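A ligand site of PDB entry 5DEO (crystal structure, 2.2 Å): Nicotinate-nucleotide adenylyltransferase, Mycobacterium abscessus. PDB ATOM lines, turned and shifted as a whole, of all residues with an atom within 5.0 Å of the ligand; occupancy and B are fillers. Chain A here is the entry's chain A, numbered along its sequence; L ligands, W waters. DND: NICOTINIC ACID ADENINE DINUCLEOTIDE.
Water W7 lies within hydrogen-bond range of an oxygen (O14) of the ligand (2.6 Å), the guanidinium group of Arg 142 (3.1 Å) and the side-chain carboxylate of Asp 117 (3.4 Å). Water W2 lies within hydrogen-bond range of an oxygen (O7N) of the ligand (2.7 Å), the backbone carbonyl oxygen of Glu 126 (2.8 Å), the backbone NH of Val 95 (3.1 Å) and the backbone NH of Thr 94 (3.3 Å). Water W9 lies within hydrogen-bond range of OG of Ser 174 (2.7 Å), O13 of the ligand (2.8 Å) and N of Phe 20 (3.3 Å). Water W8 bridges a nitrogen (N1A) of the ligand (2.8 Å) and the backbone NH of Leu 170 (3.1 Å). Water W5 lies within hydrogen-bond range of the backbone carbonyl oxygen (O) of Gly 17 (2.7 Å), an oxygen (O3B) of the ligand (2.8 Å) and the backbone carbonyl oxygen (O) of Ile 113 (2.9 Å). Water W1 bridges the side-chain hydroxyl (OG1) of Thr 94 (2.7 Å) and an oxygen (O3D) of the ligand (3.1 Å).
A ring nitrogen (ND1) of His 27 sits at hydrogen-bond distance from the backbone NH of His 24 (3.2 Å). The backbone carbonyl oxygen (O) of Thr 114 is in hydrogen-bond range of the backbone NH (N) of Val 140 (2.8 Å). The backbone NH of Gly 26 lies within hydrogen-bond range of a ring nitrogen (ND1) of His 24 (3.1 Å). O of Gly 18 lies within hydrogen-bond range of N of Thr 48. The side-chain carboxylate (OD1) of Asp 117 lies within salt-bridge range of the guanidinium group (NH1) of Arg 142 (2.8 Å). The backbone carbonyl oxygen (O) of Val 140 sits at hydrogen-bond distance from the backbone NH (N) of Ala 116, 2.9 Å away. N of Val 167 is in hydrogen-bond range of OG of Ser 141 (3.1 Å). N of Gly 18 lies within hydrogen-bond range of O of Val 46, at 3.1 Å.
Merely in contact with the ligand: Thr 48, Ser 141, Trp 125, Met 16, His 24, Ala 118, Thr 114, Tyr 93, Gly 26, Phe 112, Thr 92 and Val 140. Along chain A the residues within 4 Å of the ligand span positions 16 to 172. The nearest printed residue that does not touch the ligand is Ala 30 (4.1 Å).
N of Thr 19 is in hydrogen-bond range of O3P of the ligand, 3.3 Å away. O7N of the ligand is in hydrogen-bond range of N of Thr 94 (3.1 Å). O of Ile 172 sits at hydrogen-bond distance from N6A of the ligand. An oxygen (O8N) of the ligand is in hydrogen-bond range of the backbone NH (N) of Glu 126 (3.1 Å). OG1 of Thr 19 lies within hydrogen-bond range of O11 of the ligand (3.0 Å). The guanidinium group (NE) of Arg 142 sits close to a nitrogen (N7A) of the ligand, at 3.3 Å. O3D of the ligand sits at hydrogen-bond distance from N of Gly 18 (3.4 Å). A nitrogen (N6A) of the ligand sits at hydrogen-bond distance from the backbone carbonyl oxygen (O) of Leu 170, 3.0 Å away. The backbone NH (N) of Gly 115 sits at hydrogen-bond distance from an oxygen (O3B) of the ligand, 2.9 Å away. O13 of the ligand sits at hydrogen-bond distance from NE2 of His 27 (3.4 Å). The backbone NH (N) of Phe 20 is in hydrogen-bond range of an oxygen (O13) of the ligand, 3.4 Å away. The backbone carbonyl oxygen (O) of Gly 17 lies close to an oxygen (O3D) of the ligand, 3.5 Å away. The side-chain carboxylate of Asp 117 sits at hydrogen-bond distance from an oxygen (O2B) of the ligand, 2.7 Å away.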
ATOM      1  N   MET A  16     -20.409  13.697  -9.348  1.00  0.00           N
ATOM      2  CA  MET A  16     -20.514  13.193 -10.712  1.00  0.00           C
ATOM      3  C   MET A  16     -20.868  14.294 -11.695  1.00  0.00           C
ATOM      4  O   MET A  16     -21.995  14.763 -11.738  1.00  0.00           O
ATOM      5  CB  MET A  16     -21.520  12.084 -10.807  1.00  0.00           C
ATOM      6  CG  MET A  16     -21.546  11.513 -12.212  1.00  0.00           C
ATOM      7  SD  MET A  16     -22.098   9.830 -12.258  1.00  0.00           S
ATOM      8  CE  MET A  16     -22.559   9.810 -13.977  1.00  0.00           C
ATOM      9  N   GLY A  17     -19.895  14.688 -12.496  1.00  0.00           N
ATOM     10  CA  GLY A  17     -20.107  15.685 -13.525  1.00  0.00           C
ATOM     11  C   GLY A  17     -20.577  15.062 -14.823  1.00  0.00           C
ATOM     12  O   GLY A  17     -20.247  13.906 -15.128  1.00  0.00           O
ATOM     13  N   GLY A  18     -21.321  15.829 -15.606  1.00  0.00           N
ATOM     14  CA  GLY A  18     -21.764  15.376 -16.919  1.00  0.00           C
ATOM     15  C   GLY A  18     -22.670  16.364 -17.641  1.00  0.00           C
ATOM     16  O   GLY A  18     -23.221  17.250 -17.049  1.00  0.00           O
ATOM     17  N   THR A  19     -22.806  16.180 -18.936  1.00  0.00           N
ATOM     18  CA  THR A  19     -23.732  16.963 -19.752  1.00  0.00           C
ATOM     19  C   THR A  19     -25.179  16.591 -19.363  1.00  0.00           C
ATOM     20  O   THR A  19     -26.029  17.483 -19.250  1.00  0.00           O
ATOM     21  CB  THR A  19     -23.431  16.702 -21.237  1.00  0.00           C
ATOM     22  OG1 THR A  19     -22.016  16.777 -21.412  1.00  0.00           O
ATOM     23  CG2 THR A  19     -24.101  17.705 -22.135  1.00  0.00           C
ATOM     24  N   PHE A  20     -25.423  15.312 -19.098  1.00  0.00           N
ATOM     25  CA  PHE A  20     -26.755  14.815 -18.726  1.00  0.00           C
ATOM     26  C   PHE A  20     -27.827  15.287 -19.707  1.00  0.00           C
ATOM     27  O   PHE A  20     -28.716  16.064 -19.374  1.00  0.00           O
ATOM     28  CB  PHE A  20     -27.127  15.172 -17.283  1.00  0.00           C
ATOM     29  CG  PHE A  20     -26.112  14.699 -16.259  1.00  0.00           C
ATOM     30  CD1 PHE A  20     -25.636  13.396 -16.280  1.00  0.00           C
ATOM     31  CD2 PHE A  20     -25.633  15.571 -15.294  1.00  0.00           C
ATOM     32  CE1 PHE A  20     -24.706  12.960 -15.355  1.00  0.00           C
ATOM     33  CE2 PHE A  20     -24.699  15.159 -14.369  1.00  0.00           C
ATOM     34  CZ  PHE A  20     -24.231  13.845 -14.392  1.00  0.00           C
ATOM     35  N   HIS A  24     -29.295   9.133 -17.686  1.00  0.00           N
ATOM     36  CA  HIS A  24     -29.819   7.812 -17.906  1.00  0.00           C
ATOM     37  C   HIS A  24     -29.425   6.864 -16.769  1.00  0.00           C
ATOM     38  O   HIS A  24     -28.703   7.261 -15.828  1.00  0.00           O
ATOM     39  CB  HIS A  24     -29.431   7.275 -19.311  1.00  0.00           C
ATOM     40  CG  HIS A  24     -27.968   7.239 -19.590  1.00  0.00           C
ATOM     41  ND1 HIS A  24     -27.109   6.374 -18.951  1.00  0.00           N
ATOM     42  CD2 HIS A  24     -27.221   7.915 -20.478  1.00  0.00           C
ATOM     43  CE1 HIS A  24     -25.886   6.540 -19.404  1.00  0.00           C
ATOM     44  NE2 HIS A  24     -25.915   7.487 -20.321  1.00  0.00           N
ATOM     45  N   GLY A  26     -27.525   4.194 -16.721  1.00  0.00           N
ATOM     46  CA  GLY A  26     -26.064   4.082 -16.667  1.00  0.00           C
ATOM     47  C   GLY A  26     -25.340   5.026 -15.713  1.00  0.00           C
ATOM     48  O   GLY A  26     -24.483   4.594 -14.932  1.00  0.00           O
ATOM     49  N   HIS A  27     -25.659   6.310 -15.770  1.00  0.00           N
ATOM     50  CA  HIS A  27     -25.061   7.296 -14.874  1.00  0.00           C
ATOM     51  C   HIS A  27     -25.450   6.972 -13.428  1.00  0.00           C
ATOM     52  O   HIS A  27     -24.615   7.055 -12.526  1.00  0.00           O
ATOM     53  CB  HIS A  27     -25.572   8.708 -15.175  1.00  0.00           C
ATOM     54  CG  HIS A  27     -25.219   9.224 -16.520  1.00  0.00           C
ATOM     55  ND1 HIS A  27     -26.147   9.745 -17.392  1.00  0.00           N
ATOM     56  CD2 HIS A  27     -24.029   9.312 -17.164  1.00  0.00           C
ATOM     57  CE1 HIS A  27     -25.555  10.136 -18.504  1.00  0.00           C
ATOM     58  NE2 HIS A  27     -24.258   9.900 -18.383  1.00  0.00           N
ATOM     59  N   ALA A  30     -24.030   3.764 -11.778  1.00  0.00           N
ATOM     60  CA  ALA A  30     -22.603   3.977 -11.499  1.00  0.00           C
ATOM     61  C   ALA A  30     -22.425   4.733 -10.190  1.00  0.00           C
ATOM     62  O   ALA A  30     -21.644   4.305  -9.330  1.00  0.00           O
ATOM     63  CB  ALA A  30     -21.943   4.739 -12.622  1.00  0.00           C
ATOM     64  N   VAL A  46     -23.477  17.197 -11.048  1.00  0.00           N
ATOM     65  CA  VAL A  46     -23.182  18.536 -11.569  1.00  0.00           C
ATOM     66  C   VAL A  46     -23.350  18.566 -13.103  1.00  0.00           C
ATOM     67  O   VAL A  46     -22.437  18.164 -13.834  1.00  0.00           O
ATOM     68  CB  VAL A  46     -21.744  18.971 -11.159  1.00  0.00           C
ATOM     69  CG1 VAL A  46     -21.568  20.468 -11.376  1.00  0.00           C
ATOM     70  CG2 VAL A  46     -21.457  18.615  -9.715  1.00  0.00           C
ATOM     71  N   THR A  48     -22.925  20.142 -16.580  1.00  0.00           N
ATOM     72  CA  THR A  48     -21.994  21.130 -17.135  1.00  0.00           C
ATOM     73  C   THR A  48     -22.746  22.338 -17.657  1.00  0.00           C
ATOM     74  O   THR A  48     -23.926  22.247 -17.983  1.00  0.00           O
ATOM     75  CB  THR A  48     -21.197  20.512 -18.303  1.00  0.00           C
ATOM     76  OG1 THR A  48     -22.094  19.882 -19.214  1.00  0.00           O
ATOM     77  CG2 THR A  48     -20.223  19.482 -17.794  1.00  0.00           C
ATOM     78  N   THR A  92     -17.019  24.949 -18.854  1.00  0.00           N
ATOM     79  CA  THR A  92     -16.943  24.114 -17.654  1.00  0.00           C
ATOM     80  C   THR A  92     -15.626  23.346 -17.607  1.00  0.00           C
ATOM     81  O   THR A  92     -15.299  22.593 -18.524  1.00  0.00           O
ATOM     82  CB  THR A  92     -18.090  23.081 -17.576  1.00  0.00           C
ATOM     83  OG1 THR A  92     -19.340  23.769 -17.559  1.00  0.00           O
ATOM     84  CG2 THR A  92     -17.982  22.220 -16.323  1.00  0.00           C
ATOM     85  N   TYR A  93     -14.883  23.556 -16.523  1.00  0.00           N
ATOM     86  CA  TYR A  93     -13.683  22.785 -16.222  1.00  0.00           C
ATOM     87  C   TYR A  93     -13.864  22.164 -14.851  1.00  0.00           C
ATOM     88  O   TYR A  93     -14.383  22.818 -13.937  1.00  0.00           O
ATOM     89  CB  TYR A  93     -12.458  23.685 -16.273  1.00  0.00           C
ATOM     90  CG  TYR A  93     -12.237  24.316 -17.626  1.00  0.00           C
ATOM     91  CD1 TYR A  93     -12.092  23.529 -18.762  1.00  0.00           C
ATOM     92  CD2 TYR A  93     -12.185  25.712 -17.776  1.00  0.00           C
ATOM     93  CE1 TYR A  93     -11.906  24.093 -20.009  1.00  0.00           C
ATOM     94  CE2 TYR A  93     -11.984  26.287 -19.037  1.00  0.00           C
ATOM     95  CZ  TYR A  93     -11.850  25.468 -20.152  1.00  0.00           C
ATOM     96  OH  TYR A  93     -11.640  26.001 -21.415  1.00  0.00           O
ATOM     97  N   THR A  94     -13.451  20.916 -14.693  1.00  0.00           N
ATOM     98  CA  THR A  94     -13.633  20.194 -13.435  1.00  0.00           C
ATOM     99  C   THR A  94     -12.818  20.781 -12.277  1.00  0.00           C
ATOM    100  O   THR A  94     -13.228  20.683 -11.121  1.00  0.00           O
ATOM    101  CB  THR A  94     -13.325  18.702 -13.619  1.00  0.00           C
ATOM    102  OG1 THR A  94     -14.203  18.182 -14.617  1.00  0.00           O
ATOM    103  CG2 THR A  94     -13.558  17.909 -12.345  1.00  0.00           C
ATOM    104  N   VAL A  95     -11.695  21.427 -12.590  1.00  0.00           N
ATOM    105  CA  VAL A  95     -10.902  22.097 -11.543  1.00  0.00           C
ATOM    106  C   VAL A  95     -11.762  23.159 -10.844  1.00  0.00           C
ATOM    107  O   VAL A  95     -11.792  23.218  -9.598  1.00  0.00           O
ATOM    108  CB  VAL A  95      -9.611  22.726 -12.112  1.00  0.00           C
ATOM    109  CG1 VAL A  95      -8.903  23.542 -11.039  1.00  0.00           C
ATOM    110  CG2 VAL A  95      -8.665  21.653 -12.632  1.00  0.00           C
ATOM    111  N   PHE A 112     -14.516  12.391  -7.158  1.00  0.00           N
ATOM    112  CA  PHE A 112     -15.054  12.665  -8.478  1.00  0.00           C
ATOM    113  C   PHE A 112     -15.228  11.373  -9.261  1.00  0.00           C
ATOM    114  O   PHE A 112     -14.251  10.657  -9.514  1.00  0.00           O
ATOM    115  CB  PHE A 112     -14.149  13.611  -9.257  1.00  0.00           C
ATOM    116  CG  PHE A 112     -14.778  14.134 -10.513  1.00  0.00           C
ATOM    117  CD1 PHE A 112     -15.609  15.239 -10.466  1.00  0.00           C
ATOM    118  CD2 PHE A 112     -14.570  13.506 -11.736  1.00  0.00           C
ATOM    119  CE1 PHE A 112     -16.200  15.731 -11.619  1.00  0.00           C
ATOM    120  CE2 PHE A 112     -15.178  13.975 -12.894  1.00  0.00           C
ATOM    121  CZ  PHE A 112     -15.995  15.094 -12.836  1.00  0.00           C
ATOM    122  N   ILE A 113     -16.462  11.101  -9.679  1.00  0.00           N
ATOM    123  CA  ILE A 113     -16.816   9.858 -10.368  1.00  0.00           C
ATOM    124  C   ILE A 113     -16.789  10.044 -11.886  1.00  0.00           C
ATOM    125  O   ILE A 113     -17.418  10.961 -12.425  1.00  0.00           O
ATOM    126  CB  ILE A 113     -18.189   9.356  -9.911  1.00  0.00           C
ATOM    127  CG1 ILE A 113     -18.172   9.103  -8.396  1.00  0.00           C
ATOM    128  CG2 ILE A 113     -18.576   8.090 -10.670  1.00  0.00           C
ATOM    129  CD1 ILE A 113     -19.552   9.134  -7.784  1.00  0.00           C
ATOM    130  N   THR A 114     -16.059   9.162 -12.568  1.00  0.00           N
ATOM    131  CA  THR A 114     -15.859   9.251 -14.013  1.00  0.00           C
ATOM    132  C   THR A 114     -15.989   7.850 -14.599  1.00  0.00           C
ATOM    133  O   THR A 114     -15.536   6.888 -13.993  1.00  0.00           O
ATOM    134  CB  THR A 114     -14.475   9.840 -14.371  1.00  0.00           C
ATOM    135  OG1 THR A 114     -14.232   9.684 -15.767  1.00  0.00           O
ATOM    136  CG2 THR A 114     -13.336   9.155 -13.619  1.00  0.00           C
ATOM    137  N   GLY A 115     -16.622   7.726 -15.759  1.00  0.00           N
ATOM    138  CA  GLY A 115     -16.685   6.448 -16.484  1.00  0.00           C
ATOM    139  C   GLY A 115     -15.395   6.233 -17.266  1.00  0.00           C
ATOM    140  O   GLY A 115     -14.605   7.170 -17.464  1.00  0.00           O
ATOM    141  N   ALA A 116     -15.180   5.000 -17.689  1.00  0.00           N
ATOM    142  CA  ALA A 116     -13.956   4.591 -18.367  1.00  0.00           C
ATOM    143  C   ALA A 116     -13.559   5.513 -19.513  1.00  0.00           C
ATOM    144  O   ALA A 116     -12.377   5.831 -19.650  1.00  0.00           O
ATOM    145  CB  ALA A 116     -14.094   3.161 -18.870  1.00  0.00           C
ATOM    146  N   ASP A 117     -14.526   5.935 -20.328  1.00  0.00           N
ATOM    147  CA  ASP A 117     -14.237   6.797 -21.489  1.00  0.00           C
ATOM    148  C   ASP A 117     -13.767   8.199 -21.082  1.00  0.00           C
ATOM    149  O   ASP A 117     -12.880   8.766 -21.726  1.00  0.00           O
ATOM    150  CB  ASP A 117     -15.423   6.884 -22.485  1.00  0.00           C
ATOM    151  CG  ASP A 117     -16.655   7.568 -21.906  1.00  0.00           C
ATOM    152  OD1 ASP A 117     -17.266   7.014 -20.971  1.00  0.00           O
ATOM    153  OD2 ASP A 117     -17.019   8.657 -22.409  1.00  0.00           O
ATOM    154  N   ALA A 118     -14.364   8.728 -20.019  1.00  0.00           N
ATOM    155  CA  ALA A 118     -13.988  10.041 -19.494  1.00  0.00           C
ATOM    156  C   ALA A 118     -12.629  10.008 -18.814  1.00  0.00           C
ATOM    157  O   ALA A 118     -11.813  10.905 -19.040  1.00  0.00           O
ATOM    158  CB  ALA A 118     -15.045  10.572 -18.532  1.00  0.00           C
ATOM    159  N   SER A 124      -6.063  15.502 -21.164  1.00  0.00           N
ATOM    160  CA  SER A 124      -6.421  16.682 -21.957  1.00  0.00           C
ATOM    161  C   SER A 124      -7.230  17.725 -21.170  1.00  0.00           C
ATOM    162  O   SER A 124      -7.527  18.797 -21.700  1.00  0.00           O
ATOM    163  CB  SER A 124      -7.221  16.239 -23.174  1.00  0.00           C
ATOM    164  OG  SER A 124      -8.467  15.673 -22.768  1.00  0.00           O
ATOM    165  N   TRP A 125      -7.578  17.436 -19.912  1.00  0.00           N
ATOM    166  CA  TRP A 125      -8.380  18.353 -19.102  1.00  0.00           C
ATOM    167  C   TRP A 125      -7.562  19.558 -18.626  1.00  0.00           C
ATOM    168  O   TRP A 125      -6.379  19.427 -18.312  1.00  0.00           O
ATOM    169  CB  TRP A 125      -8.987  17.633 -17.891  1.00  0.00           C
ATOM    170  CG  TRP A 125      -9.984  16.572 -18.208  1.00  0.00           C
ATOM    171  CD1 TRP A 125     -10.204  15.960 -19.418  1.00  0.00           C
ATOM    172  CD2 TRP A 125     -10.896  15.958 -17.292  1.00  0.00           C
ATOM    173  NE1 TRP A 125     -11.185  15.020 -19.303  1.00  0.00           N
ATOM    174  CE2 TRP A 125     -11.635  15.003 -18.009  1.00  0.00           C
ATOM    175  CE3 TRP A 125     -11.162  16.138 -15.928  1.00  0.00           C
ATOM    176  CZ2 TRP A 125     -12.626  14.212 -17.417  1.00  0.00           C
ATOM    177  CZ3 TRP A 125     -12.148  15.350 -15.328  1.00  0.00           C
ATOM    178  CH2 TRP A 125     -12.874  14.403 -16.083  1.00  0.00           C
ATOM    179  N   GLU A 126      -8.193  20.728 -18.620  1.00  0.00           N
ATOM    180  CA  GLU A 126      -7.615  21.954 -18.085  1.00  0.00           C
ATOM    181  C   GLU A 126      -6.894  21.706 -16.764  1.00  0.00           C
ATOM    182  O   GLU A 126      -7.497  21.163 -15.827  1.00  0.00           O
ATOM    183  CB  GLU A 126      -8.718  23.003 -17.885  1.00  0.00           C
ATOM    184  CG  GLU A 126      -8.220  24.424 -17.584  1.00  0.00           C
ATOM    185  CD  GLU A 126      -7.690  25.167 -18.801  1.00  0.00           C
ATOM    186  OE1 GLU A 126      -7.598  24.571 -19.903  1.00  0.00           O
ATOM    187  OE2 GLU A 126      -7.356  26.356 -18.649  1.00  0.00           O
ATOM    188  N   VAL A 140     -15.174   4.233 -13.121  1.00  0.00           N
ATOM    189  CA  VAL A 140     -16.130   3.136 -13.153  1.00  0.00           C
ATOM    190  C   VAL A 140     -16.131   2.517 -14.542  1.00  0.00           C
ATOM    191  O   VAL A 140     -15.882   3.208 -15.549  1.00  0.00           O
ATOM    192  CB  VAL A 140     -17.564   3.566 -12.776  1.00  0.00           C
ATOM    193  CG1 VAL A 140     -17.600   4.091 -11.359  1.00  0.00           C
ATOM    194  CG2 VAL A 140     -18.136   4.591 -13.740  1.00  0.00           C
ATOM    195  N   SER A 141     -16.422   1.221 -14.588  1.00  0.00           N
ATOM    196  CA  SER A 141     -16.500   0.502 -15.867  1.00  0.00           C
ATOM    197  C   SER A 141     -17.675   1.008 -16.699  1.00  0.00           C
ATOM    198  O   SER A 141     -18.647   1.587 -16.183  1.00  0.00           O
ATOM    199  CB  SER A 141     -16.621  -1.013 -15.669  1.00  0.00           C
ATOM    200  OG  SER A 141     -17.743  -1.344 -14.866  1.00  0.00           O
ATOM    201  N   ARG A 142     -17.568   0.789 -17.997  1.00  0.00           N
ATOM    202  CA  ARG A 142     -18.599   1.160 -18.940  1.00  0.00           C
ATOM    203  C   ARG A 142     -18.474   0.258 -20.182  1.00  0.00           C
ATOM    204  O   ARG A 142     -17.385   0.143 -20.732  1.00  0.00           O
ATOM    205  CB  ARG A 142     -18.458   2.619 -19.324  1.00  0.00           C
ATOM    206  CG  ARG A 142     -19.552   3.088 -20.263  1.00  0.00           C
ATOM    207  CD  ARG A 142     -19.367   4.498 -20.736  1.00  0.00           C
ATOM    208  NE  ARG A 142     -20.484   4.841 -21.631  1.00  0.00           N
ATOM    209  CZ  ARG A 142     -20.720   6.049 -22.133  1.00  0.00           C
ATOM    210  NH1 ARG A 142     -19.929   7.076 -21.861  1.00  0.00           N
ATOM    211  NH2 ARG A 142     -21.773   6.218 -22.921  1.00  0.00           N
ATOM    212  N   PRO A 143     -19.579  -0.401 -20.607  1.00  0.00           N
ATOM    213  CA  PRO A 143     -19.503  -1.331 -21.749  1.00  0.00           C
ATOM    214  C   PRO A 143     -18.999  -0.659 -23.009  1.00  0.00           C
ATOM    215  O   PRO A 143     -19.375   0.489 -23.281  1.00  0.00           O
ATOM    216  CB  PRO A 143     -20.951  -1.807 -21.927  1.00  0.00           C
ATOM    217  CG  PRO A 143     -21.544  -1.634 -20.572  1.00  0.00           C
ATOM    218  CD  PRO A 143     -20.947  -0.378 -20.038  1.00  0.00           C
ATOM    219  N   VAL A 167     -18.848  -1.583 -12.018  1.00  0.00           N
ATOM    220  CA  VAL A 167     -20.267  -1.306 -11.730  1.00  0.00           C
ATOM    221  C   VAL A 167     -21.102  -2.128 -12.708  1.00  0.00           C
ATOM    222  O   VAL A 167     -20.562  -2.568 -13.742  1.00  0.00           O
ATOM    223  CB  VAL A 167     -20.597   0.190 -11.832  1.00  0.00           C
ATOM    224  CG1 VAL A 167     -19.592   0.990 -11.005  1.00  0.00           C
ATOM    225  CG2 VAL A 167     -20.610   0.668 -13.289  1.00  0.00           C
ATOM    226  N   LEU A 170     -24.497  -1.558 -17.914  1.00  0.00           N
ATOM    227  CA  LEU A 170     -25.655  -1.080 -18.667  1.00  0.00           C
ATOM    228  C   LEU A 170     -25.173  -0.328 -19.893  1.00  0.00           C
ATOM    229  O   LEU A 170     -24.664   0.803 -19.777  1.00  0.00           O
ATOM    230  CB  LEU A 170     -26.547  -0.190 -17.794  1.00  0.00           C
ATOM    231  CG  LEU A 170     -26.956  -0.683 -16.405  1.00  0.00           C
ATOM    232  CD1 LEU A 170     -27.988   0.268 -15.849  1.00  0.00           C
ATOM    233  CD2 LEU A 170     -27.508  -2.095 -16.384  1.00  0.00           C
ATOM    234  N   ILE A 172     -25.849   1.814 -22.157  1.00  0.00           N
ATOM    235  CA  ILE A 172     -26.741   2.919 -22.418  1.00  0.00           C
ATOM    236  C   ILE A 172     -25.843   4.131 -22.655  1.00  0.00           C
ATOM    237  O   ILE A 172     -24.913   4.365 -21.871  1.00  0.00           O
ATOM    238  CB  ILE A 172     -27.637   3.162 -21.189  1.00  0.00           C
ATOM    239  CG1 ILE A 172     -28.294   1.845 -20.743  1.00  0.00           C
ATOM    240  CG2 ILE A 172     -28.679   4.234 -21.484  1.00  0.00           C
ATOM    241  CD1 ILE A 172     -29.253   1.985 -19.567  1.00  0.00           C
ATOM    242  N   SER A 174     -26.236   8.483 -23.758  1.00  0.00           N
ATOM    243  CA  SER A 174     -27.104   9.610 -23.993  1.00  0.00           C
ATOM    244  C   SER A 174     -27.338   9.787 -25.490  1.00  0.00           C
ATOM    245  O   SER A 174     -28.445  10.149 -25.905  1.00  0.00           O
ATOM    246  CB  SER A 174     -26.537  10.893 -23.397  1.00  0.00           C
ATOM    247  OG  SER A 174     -26.527  10.799 -21.984  1.00  0.00           O
HETATM  248  PN  DND L   1     -19.342  14.018 -20.265  1.00  0.00           P
HETATM  249  O11 DND L   1     -19.643  14.884 -21.421  1.00  0.00           O
HETATM  250  O12 DND L   1     -18.679  12.732 -20.688  1.00  0.00           O
HETATM  251  O3P DND L   1     -20.733  13.670 -19.588  1.00  0.00           O
HETATM  252  O5D DND L   1     -18.374  14.735 -19.208  1.00  0.00           O
HETATM  253  C5D DND L   1     -17.878  13.988 -18.073  1.00  0.00           C
HETATM  254  C4D DND L   1     -17.245  14.930 -17.092  1.00  0.00           C
HETATM  255  O4D DND L   1     -15.923  15.274 -17.549  1.00  0.00           O
HETATM  256  C3D DND L   1     -17.985  16.263 -16.882  1.00  0.00           C
HETATM  257  O3D DND L   1     -18.040  16.577 -15.491  1.00  0.00           O
HETATM  258  C2D DND L   1     -17.124  17.263 -17.639  1.00  0.00           C
HETATM  259  O2D DND L   1     -17.173  18.585 -17.113  1.00  0.00           O
HETATM  260  C1D DND L   1     -15.754  16.649 -17.410  1.00  0.00           C
HETATM  261  N1N DND L   1     -14.699  17.119 -18.393  1.00  0.00           N
HETATM  262  C6N DND L   1     -14.819  16.809 -19.699  1.00  0.00           C
HETATM  263  C5N DND L   1     -13.990  17.413 -20.615  1.00  0.00           C
HETATM  264  C4N DND L   1     -13.039  18.326 -20.189  1.00  0.00           C
HETATM  265  C3N DND L   1     -12.914  18.601 -18.820  1.00  0.00           C
HETATM  266  C2N DND L   1     -13.751  17.966 -17.936  1.00  0.00           C
HETATM  267  C7N DND L   1     -11.944  19.609 -18.317  1.00  0.00           C
HETATM  268  O7N DND L   1     -11.854  19.859 -17.134  1.00  0.00           O
HETATM  269  O8N DND L   1     -11.207  20.150 -19.207  1.00  0.00           O
HETATM  270  PA  DND L   1     -21.730  12.443 -19.835  1.00  0.00           P
HETATM  271  O13 DND L   1     -23.100  12.865 -19.475  1.00  0.00           O
HETATM  272  O14 DND L   1     -21.599  12.067 -21.280  1.00  0.00           O
HETATM  273  O5B DND L   1     -21.238  11.297 -18.905  1.00  0.00           O
HETATM  274  C5B DND L   1     -21.196  11.478 -17.475  1.00  0.00           C
HETATM  275  C4B DND L   1     -20.288  10.442 -16.878  1.00  0.00           C
HETATM  276  O4B DND L   1     -20.947   9.163 -16.863  1.00  0.00           O
HETATM  277  C3B DND L   1     -18.967  10.253 -17.627  1.00  0.00           C
HETATM  278  O3B DND L   1     -17.909  10.216 -16.677  1.00  0.00           O
HETATM  279  C2B DND L   1     -19.198   8.947 -18.403  1.00  0.00           C
HETATM  280  O2B DND L   1     -17.999   8.223 -18.629  1.00  0.00           O
HETATM  281  C1B DND L   1     -20.105   8.187 -17.442  1.00  0.00           C
HETATM  282  N9A DND L   1     -20.949   7.166 -18.068  1.00  0.00           N
HETATM  283  C4A DND L   1     -21.151   5.874 -17.633  1.00  0.00           C
HETATM  284  N3A DND L   1     -20.516   5.236 -16.657  1.00  0.00           N
HETATM  285  C2A DND L   1     -20.931   3.966 -16.561  1.00  0.00           C
HETATM  286  N1A DND L   1     -21.848   3.322 -17.296  1.00  0.00           N
HETATM  287  C6A DND L   1     -22.481   4.005 -18.279  1.00  0.00           C
HETATM  288  C5A DND L   1     -22.123   5.355 -18.473  1.00  0.00           C
HETATM  289  N7A DND L   1     -22.509   6.286 -19.427  1.00  0.00           N
HETATM  290  C8A DND L   1     -21.777   7.336 -19.149  1.00  0.00           C
HETATM  291  N6A DND L   1     -23.403   3.378 -18.992  1.00  0.00           N
HETATM  292  O   HOH W   1     -16.670  18.934 -13.949  1.00  0.00           O
HETATM  293  O   HOH W   2     -10.196  20.818 -15.215  1.00  0.00           O
HETATM  294  O   HOH W   3     -19.705  18.922 -14.541  1.00  0.00           O
HETATM  295  O   HOH W   4     -18.052  17.650 -22.478  1.00  0.00           O
HETATM  296  O   HOH W   5     -17.993  12.373 -14.867  1.00  0.00           O
HETATM  297  O   HOH W   6     -16.484  20.177 -19.053  1.00  0.00           O
HETATM  298  O   HOH W   7     -19.981  10.166 -21.891  1.00  0.00           O
HETATM  299  O   HOH W   8     -22.557   0.638 -16.881  1.00  0.00           O
HETATM  300  O   HOH W   9     -25.061  12.948 -21.411  1.00  0.00           O
